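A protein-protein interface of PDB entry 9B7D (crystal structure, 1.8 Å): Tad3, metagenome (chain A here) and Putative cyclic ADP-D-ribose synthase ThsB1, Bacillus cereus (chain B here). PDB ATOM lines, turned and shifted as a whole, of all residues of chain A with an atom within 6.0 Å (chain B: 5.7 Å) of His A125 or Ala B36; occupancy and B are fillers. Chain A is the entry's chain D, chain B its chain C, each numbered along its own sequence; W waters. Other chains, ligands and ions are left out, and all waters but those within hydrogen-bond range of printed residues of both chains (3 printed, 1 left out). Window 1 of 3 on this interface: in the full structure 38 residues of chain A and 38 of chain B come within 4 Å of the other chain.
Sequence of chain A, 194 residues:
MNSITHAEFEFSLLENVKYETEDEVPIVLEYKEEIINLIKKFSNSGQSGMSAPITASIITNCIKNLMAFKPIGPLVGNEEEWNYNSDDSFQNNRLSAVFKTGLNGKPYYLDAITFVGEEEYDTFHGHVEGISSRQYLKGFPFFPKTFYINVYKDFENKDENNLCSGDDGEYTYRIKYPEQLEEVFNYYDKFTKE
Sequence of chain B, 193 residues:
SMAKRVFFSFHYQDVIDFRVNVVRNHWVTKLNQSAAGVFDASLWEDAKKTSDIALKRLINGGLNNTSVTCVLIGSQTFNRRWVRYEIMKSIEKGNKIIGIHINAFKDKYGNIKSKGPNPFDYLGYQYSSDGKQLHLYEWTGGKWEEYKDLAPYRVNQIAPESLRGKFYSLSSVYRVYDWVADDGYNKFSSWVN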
ATOM      1  N   LEU A 110       1.146   2.468   1.877  1.00  0.00           N
ATOM      2  CA  LEU A 110       2.072   1.679   2.690  1.00  0.00           C
ATOM      3  C   LEU A 110       2.528   2.418   3.941  1.00  0.00           C
ATOM      4  O   LEU A 110       2.916   1.779   4.927  1.00  0.00           O
ATOM      5  CB  LEU A 110       3.302   1.279   1.877  1.00  0.00           C
ATOM      6  CG  LEU A 110       3.134   0.354   0.672  1.00  0.00           C
ATOM      7  CD1 LEU A 110       4.512  -0.086   0.202  1.00  0.00           C
ATOM      8  CD2 LEU A 110       2.271  -0.838   1.031  1.00  0.00           C
ATOM      9  N   ASP A 111       2.512   3.750   3.918  1.00  0.00           N
ATOM     10  CA  ASP A 111       3.113   4.559   4.973  1.00  0.00           C
ATOM     11  C   ASP A 111       2.085   5.192   5.906  1.00  0.00           C
ATOM     12  O   ASP A 111       2.404   6.174   6.585  1.00  0.00           O
ATOM     13  CB  ASP A 111       3.991   5.651   4.361  1.00  0.00           C
ATOM     14  CG  ASP A 111       5.144   5.088   3.559  1.00  0.00           C
ATOM     15  OD1 ASP A 111       5.538   3.932   3.819  1.00  0.00           O
ATOM     16  OD2 ASP A 111       5.654   5.803   2.673  1.00  0.00           O
ATOM     17  N   ALA A 112       0.866   4.645   5.962  1.00  0.00           N
ATOM     18  CA  ALA A 112      -0.187   5.249   6.779  1.00  0.00           C
ATOM     19  C   ALA A 112       0.201   5.308   8.254  1.00  0.00           C
ATOM     20  O   ALA A 112      -0.091   6.297   8.944  1.00  0.00           O
ATOM     21  CB  ALA A 112      -1.494   4.472   6.600  1.00  0.00           C
ATOM     22  N   ILE A 113       0.867   4.273   8.759  1.00  0.00           N
ATOM     23  CA  ILE A 113       1.200   4.176  10.174  1.00  0.00           C
ATOM     24  C   ILE A 113       2.661   3.779  10.319  1.00  0.00           C
ATOM     25  O   ILE A 113       3.095   2.780   9.736  1.00  0.00           O
ATOM     26  CB  ILE A 113       0.302   3.155  10.898  1.00  0.00           C
ATOM     27  CG1 ILE A 113      -1.120   3.697  11.046  1.00  0.00           C
ATOM     28  CG2 ILE A 113       0.899   2.796  12.259  1.00  0.00           C
ATOM     29  CD1 ILE A 113      -2.140   2.636  11.443  1.00  0.00           C
ATOM     30  N   THR A 114       3.414   4.554  11.092  1.00  0.00           N
ATOM     31  CA  THR A 114       4.701   4.124  11.623  1.00  0.00           C
ATOM     32  C   THR A 114       4.526   3.813  13.103  1.00  0.00           C
ATOM     33  O   THR A 114       3.934   4.608  13.839  1.00  0.00           O
ATOM     34  CB  THR A 114       5.782   5.196  11.440  1.00  0.00           C
ATOM     35  OG1 THR A 114       6.059   5.379  10.044  1.00  0.00           O
ATOM     36  CG2 THR A 114       7.062   4.775  12.149  1.00  0.00           C
ATOM     37  N   PHE A 115       5.030   2.663  13.540  1.00  0.00           N
ATOM     38  CA  PHE A 115       4.923   2.282  14.945  1.00  0.00           C
ATOM     39  C   PHE A 115       6.129   2.779  15.734  1.00  0.00           C
ATOM     40  O   PHE A 115       7.264   2.731  15.252  1.00  0.00           O
ATOM     41  CB  PHE A 115       4.792   0.769  15.079  1.00  0.00           C
ATOM     42  CG  PHE A 115       3.515   0.230  14.515  1.00  0.00           C
ATOM     43  CD1 PHE A 115       2.302   0.500  15.133  1.00  0.00           C
ATOM     44  CD2 PHE A 115       3.521  -0.528  13.353  1.00  0.00           C
ATOM     45  CE1 PHE A 115       1.118   0.003  14.615  1.00  0.00           C
ATOM     46  CE2 PHE A 115       2.339  -1.025  12.823  1.00  0.00           C
ATOM     47  CZ  PHE A 115       1.139  -0.765  13.459  1.00  0.00           C
ATOM     48  N   TYR A 121      14.716   4.826  19.168  1.00  0.00           N
ATOM     49  CA  TYR A 121      15.058   4.255  17.864  1.00  0.00           C
ATOM     50  C   TYR A 121      14.215   3.036  17.499  1.00  0.00           C
ATOM     51  O   TYR A 121      14.407   2.487  16.406  1.00  0.00           O
ATOM     52  CB  TYR A 121      16.542   3.870  17.749  1.00  0.00           C
ATOM     53  CG  TYR A 121      17.496   4.941  18.230  1.00  0.00           C
ATOM     54  CD1 TYR A 121      17.557   6.178  17.600  1.00  0.00           C
ATOM     55  CD2 TYR A 121      18.351   4.706  19.299  1.00  0.00           C
ATOM     56  CE1 TYR A 121      18.438   7.157  18.032  1.00  0.00           C
ATOM     57  CE2 TYR A 121      19.231   5.675  19.738  1.00  0.00           C
ATOM     58  CZ  TYR A 121      19.271   6.896  19.102  1.00  0.00           C
ATOM     59  OH  TYR A 121      20.153   7.859  19.542  1.00  0.00           O
ATOM     60  N   ASP A 122      13.289   2.596  18.352  1.00  0.00           N
ATOM     61  CA  ASP A 122      12.484   1.410  18.057  1.00  0.00           C
ATOM     62  C   ASP A 122      11.242   1.825  17.268  1.00  0.00           C
ATOM     63  O   ASP A 122      10.109   1.795  17.749  1.00  0.00           O
ATOM     64  CB  ASP A 122      12.110   0.678  19.341  1.00  0.00           C
ATOM     65  CG  ASP A 122      11.503  -0.689  19.066  1.00  0.00           C
ATOM     66  OD1 ASP A 122      11.785  -1.242  17.981  1.00  0.00           O
ATOM     67  OD2 ASP A 122      10.735  -1.201  19.911  1.00  0.00           O
ATOM     68  N   THR A 123      11.482   2.218  16.020  1.00  0.00           N
ATOM     69  CA  THR A 123      10.434   2.717  15.137  1.00  0.00           C
ATOM     70  C   THR A 123      10.421   1.875  13.870  1.00  0.00           C
ATOM     71  O   THR A 123      11.480   1.602  13.295  1.00  0.00           O
ATOM     72  CB  THR A 123      10.662   4.193  14.812  1.00  0.00           C
ATOM     73  OG1 THR A 123      11.986   4.374  14.287  1.00  0.00           O
ATOM     74  CG2 THR A 123      10.522   5.027  16.081  1.00  0.00           C
ATOM     75  N   PHE A 124       9.231   1.458  13.436  1.00  0.00           N
ATOM     76  CA  PHE A 124       9.196   0.435  12.402  1.00  0.00           C
ATOM     77  C   PHE A 124       7.866   0.431  11.660  1.00  0.00           C
ATOM     78  O   PHE A 124       6.859   0.959  12.134  1.00  0.00           O
ATOM     79  CB  PHE A 124       9.469  -0.949  13.001  1.00  0.00           C
ATOM     80  CG  PHE A 124       8.466  -1.381  14.045  1.00  0.00           C
ATOM     81  CD1 PHE A 124       8.570  -0.940  15.359  1.00  0.00           C
ATOM     82  CD2 PHE A 124       7.440  -2.259  13.722  1.00  0.00           C
ATOM     83  CE1 PHE A 124       7.658  -1.357  16.328  1.00  0.00           C
ATOM     84  CE2 PHE A 124       6.523  -2.677  14.687  1.00  0.00           C
ATOM     85  CZ  PHE A 124       6.637  -2.225  15.987  1.00  0.00           C
ATOM     86  N   HIS A 125       7.895  -0.168  10.473  1.00  0.00           N
ATOM     87  CA  HIS A 125       6.702  -0.575   9.750  1.00  0.00           C
ATOM     88  C   HIS A 125       6.436  -2.048  10.035  1.00  0.00           C
ATOM     89  O   HIS A 125       7.371  -2.843  10.148  1.00  0.00           O
ATOM     90  CB  HIS A 125       6.884  -0.353   8.246  1.00  0.00           C
ATOM     91  CG  HIS A 125       6.861   1.087   7.847  1.00  0.00           C
ATOM     92  ND1 HIS A 125       7.866   1.671   7.103  1.00  0.00           N
ATOM     93  CD2 HIS A 125       5.953   2.063   8.086  1.00  0.00           C
ATOM     94  CE1 HIS A 125       7.578   2.945   6.905  1.00  0.00           C
ATOM     95  NE2 HIS A 125       6.420   3.207   7.487  1.00  0.00           N
ATOM     96  N   GLY A 126       5.163  -2.409  10.167  1.00  0.00           N
ATOM     97  CA  GLY A 126       4.828  -3.800  10.440  1.00  0.00           C
ATOM     98  C   GLY A 126       3.355  -3.974  10.736  1.00  0.00           C
ATOM     99  O   GLY A 126       2.509  -3.230  10.225  1.00  0.00           O
ATOM    100  N   HIS A 127       3.060  -4.981  11.561  1.00  0.00           N
ATOM    101  CA  HIS A 127       1.711  -5.312  12.013  1.00  0.00           C
ATOM    102  C   HIS A 127       1.733  -5.392  13.531  1.00  0.00           C
ATOM    103  O   HIS A 127       2.568  -6.099  14.098  1.00  0.00           O
ATOM    104  CB  HIS A 127       1.239  -6.670  11.470  1.00  0.00           C
ATOM    105  CG  HIS A 127       0.875  -6.673  10.018  1.00  0.00           C
ATOM    106  ND1 HIS A 127      -0.369  -7.061   9.567  1.00  0.00           N
ATOM    107  CD2 HIS A 127       1.598  -6.371   8.913  1.00  0.00           C
ATOM    108  CE1 HIS A 127      -0.400  -6.987   8.248  1.00  0.00           C
ATOM    109  NE2 HIS A 127       0.781  -6.569   7.826  1.00  0.00           N
ATOM    110  N   SER A 133       0.771  -1.292   8.950  1.00  0.00           N
ATOM    111  CA  SER A 133       1.270   0.008   8.523  1.00  0.00           C
ATOM    112  C   SER A 133       0.509   0.503   7.302  1.00  0.00           C
ATOM    113  O   SER A 133       0.260   1.705   7.164  1.00  0.00           O
ATOM    114  CB  SER A 133       2.772  -0.066   8.233  1.00  0.00           C
ATOM    115  OG  SER A 133       3.506  -0.047   9.446  1.00  0.00           O
ATOM    116  N   ARG B  24       8.618  -3.310  -0.876  1.00  0.00           N
ATOM    117  CA  ARG B  24       7.930  -3.149   0.403  1.00  0.00           C
ATOM    118  C   ARG B  24       6.497  -3.655   0.332  1.00  0.00           C
ATOM    119  O   ARG B  24       5.980  -4.220   1.303  1.00  0.00           O
ATOM    120  CB  ARG B  24       7.948  -1.683   0.842  1.00  0.00           C
ATOM    121  CG  ARG B  24       9.306  -1.173   1.272  1.00  0.00           C
ATOM    122  CD  ARG B  24       9.222   0.292   1.666  1.00  0.00           C
ATOM    123  NE  ARG B  24       8.344   0.474   2.815  1.00  0.00           N
ATOM    124  CZ  ARG B  24       7.484   1.474   2.956  1.00  0.00           C
ATOM    125  NH1 ARG B  24       7.357   2.416   2.033  1.00  0.00           N
ATOM    126  NH2 ARG B  24       6.734   1.535   4.052  1.00  0.00           N
ATOM    127  N   ASN B  32       6.703  -9.787   9.365  1.00  0.00           N
ATOM    128  CA  ASN B  32       7.745  -9.053   8.663  1.00  0.00           C
ATOM    129  C   ASN B  32       7.696  -7.593   9.087  1.00  0.00           C
ATOM    130  O   ASN B  32       6.677  -6.922   8.890  1.00  0.00           O
ATOM    131  CB  ASN B  32       7.573  -9.182   7.148  1.00  0.00           C
ATOM    132  CG  ASN B  32       7.513 -10.631   6.683  1.00  0.00           C
ATOM    133  OD1 ASN B  32       6.784 -10.962   5.749  1.00  0.00           O
ATOM    134  ND2 ASN B  32       8.276 -11.501   7.340  1.00  0.00           N
ATOM    135  N   GLN B  33       8.787  -7.109   9.675  1.00  0.00           N
ATOM    136  CA  GLN B  33       8.932  -5.712  10.051  1.00  0.00           C
ATOM    137  C   GLN B  33      10.101  -5.102   9.294  1.00  0.00           C
ATOM    138  O   GLN B  33      10.995  -5.807   8.822  1.00  0.00           O
ATOM    139  CB  GLN B  33       9.172  -5.551  11.555  1.00  0.00           C
ATOM    140  CG  GLN B  33       8.090  -6.164  12.427  1.00  0.00           C
ATOM    141  CD  GLN B  33       8.394  -6.015  13.901  1.00  0.00           C
ATOM    142  OE1 GLN B  33       9.461  -5.529  14.279  1.00  0.00           O
ATOM    143  NE2 GLN B  33       7.459  -6.440  14.746  1.00  0.00           N
ATOM    144  N   SER B  34      10.097  -3.777   9.190  1.00  0.00           N
ATOM    145  CA  SER B  34      11.229  -3.063   8.619  1.00  0.00           C
ATOM    146  C   SER B  34      11.469  -1.788   9.413  1.00  0.00           C
ATOM    147  O   SER B  34      10.521  -1.158   9.888  1.00  0.00           O
ATOM    148  CB  SER B  34      11.010  -2.753   7.130  1.00  0.00           C
ATOM    149  OG  SER B  34       9.892  -1.910   6.911  1.00  0.00           O
ATOM    150  N   ALA B  35      12.743  -1.425   9.569  1.00  0.00           N
ATOM    151  CA  ALA B  35      13.085  -0.206  10.294  1.00  0.00           C
ATOM    152  C   ALA B  35      12.557   1.018   9.560  1.00  0.00           C
ATOM    153  O   ALA B  35      12.577   1.083   8.328  1.00  0.00           O
ATOM    154  CB  ALA B  35      14.598  -0.091  10.471  1.00  0.00           C
ATOM    155  N   ALA B  36      12.093   2.001  10.329  1.00  0.00           N
ATOM    156  CA  ALA B  36      11.537   3.224   9.770  1.00  0.00           C
ATOM    157  C   ALA B  36      11.915   4.393  10.663  1.00  0.00           C
ATOM    158  O   ALA B  36      11.835   4.289  11.889  1.00  0.00           O
ATOM    159  CB  ALA B  36      10.010   3.132   9.641  1.00  0.00           C
ATOM    160  N   GLY B  37      12.327   5.507  10.049  1.00  0.00           N
ATOM    161  CA  GLY B  37      12.681   6.694  10.806  1.00  0.00           C
ATOM    162  C   GLY B  37      11.478   7.523  11.237  1.00  0.00           C
ATOM    163  O   GLY B  37      10.359   7.362  10.748  1.00  0.00           O
ATOM    164  N   VAL B  38      11.729   8.449  12.166  1.00  0.00           N
ATOM    165  CA  VAL B  38      10.665   9.201  12.828  1.00  0.00           C
ATOM    166  C   VAL B  38      11.114  10.645  13.089  1.00  0.00           C
ATOM    167  O   VAL B  38      10.325  11.491  13.530  1.00  0.00           O
ATOM    168  CB  VAL B  38      10.240   8.436  14.106  1.00  0.00           C
ATOM    169  CG1 VAL B  38       9.694   9.322  15.199  1.00  0.00           C
ATOM    170  CG2 VAL B  38       9.189   7.377  13.752  1.00  0.00           C
HETATM  171  O   HOH W   1       8.435   6.630   9.337  1.00  0.00           O
HETATM  172  O   HOH W   2      10.564   0.634   6.444  1.00  0.00           O
HETATM  173  O   HOH W   3       4.950  -6.885  12.399  1.00  0.00           O
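Of the printed residues of chain B, Leu A110 touches Arg B24 (3.8 Å). Printed residues of chain B within 4 Å of Thr A114: Val B38 (3.7 Å). Of the printed residues of chain B, Thr A123 touches Ala B35, Ala B36 and Val B38. His A125 touches just these residues of chain B: Arg B24, Gln B33, Ser B34 and Ala B36. Printed residues of chain A within 4 Å of Gln B33: Phe A124 (3.9 Å) and His A125 (3.3 Å). Of the printed residues of chain A, Ala B36 touches Thr A123 (2.4 Å), Phe A124 (3.9 Å) and His A125 (3.6 Å). The nearest residue of chain A that does not touch Ala B36 is Thr A114 (4.2 Å). The nearest printed residue of chain B that does not touch Thr A123 is Gly B37 (4.2 Å).
OG1 of Thr A123 sits at hydrogen-bond distance from O of Ala B36, 2.4 Å away. NH2 of Arg B24 is in hydrogen-bond range of ND1 of His A125, at 3.3 Å. The backbone NH (N) of His A125 lies within hydrogen-bond range of the backbone carbonyl oxygen (O) of Ser B34. NH2 of Arg B24 lies within salt-bridge range of OD1 of Asp A111, 2.7 Å away.
Leu A110 touches Arg B24. Val B38 touches Thr A114. Thr A123 touches Ala B35 (O to CA, 3.9 Å). CG2 of Thr A123 touches CG2 of Val B38, 3.6 Å away. Gln B33 touches Phe A124 (NE2 to CE2, 3.9 Å). O of Ser B34 touches CA of Phe A124, 3.3 Å away. N of Ala B36 touches CA of Phe A124, at 3.9 Å. Gln B33 touches His A125 (CA to O, 3.3 Å). CB of Ala B36 touches ND1 of His A125, 3.6 Å away. Gly A126 touches Asn B32.
OG1 of Thr A114 lies within hydrogen-bond range of NE2 of His A125 (3.4 Å). The backbone NH (N) of Phe A115 lies within hydrogen-bond range of the backbone carbonyl oxygen (O) of Phe A124, 2.9 Å away. O of Gly A126 is in hydrogen-bond range of N of Ser A133 (2.9 Å).
Water W1 lies within hydrogen-bond range of the backbone carbonyl oxygen of Gly B37 (2.5 Å) and the side-chain hydroxyl of Thr A114 (2.8 Å). Water W2 lies within hydrogen-bond range of OG of Ser B34 (2.7 Å), O of Ala B35 (2.8 Å) and ND1 of His A125 (3.0 Å). Water W3 bridges the backbone NH (N) of His A127 (2.8 Å) and the side-chain amide nitrogen (NE2) of Gln B33 (3.5 Å).
Of the 8 printed residues of chain B, 7 touch a printed residue of chain A. Hydrophobic or aromatic side chains of chain B within 4 Å of the printed part of chain A: Ala B36 and Val B38. Printed residues of chain A that touch a printed residue of chain B: Leu A110, Asp A111, Thr A114, Thr A123, Phe A124, His A125 and Gly A126. Hydrophobic or aromatic side chains of chain A that line the printed part of chain B: Leu A110, Phe A124 and His A125. Among the printed residues, Asp or Glu carboxylates within 4 Å of a Lys or Arg side-chain nitrogen of the other chain: Asp A111 with Arg B24.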
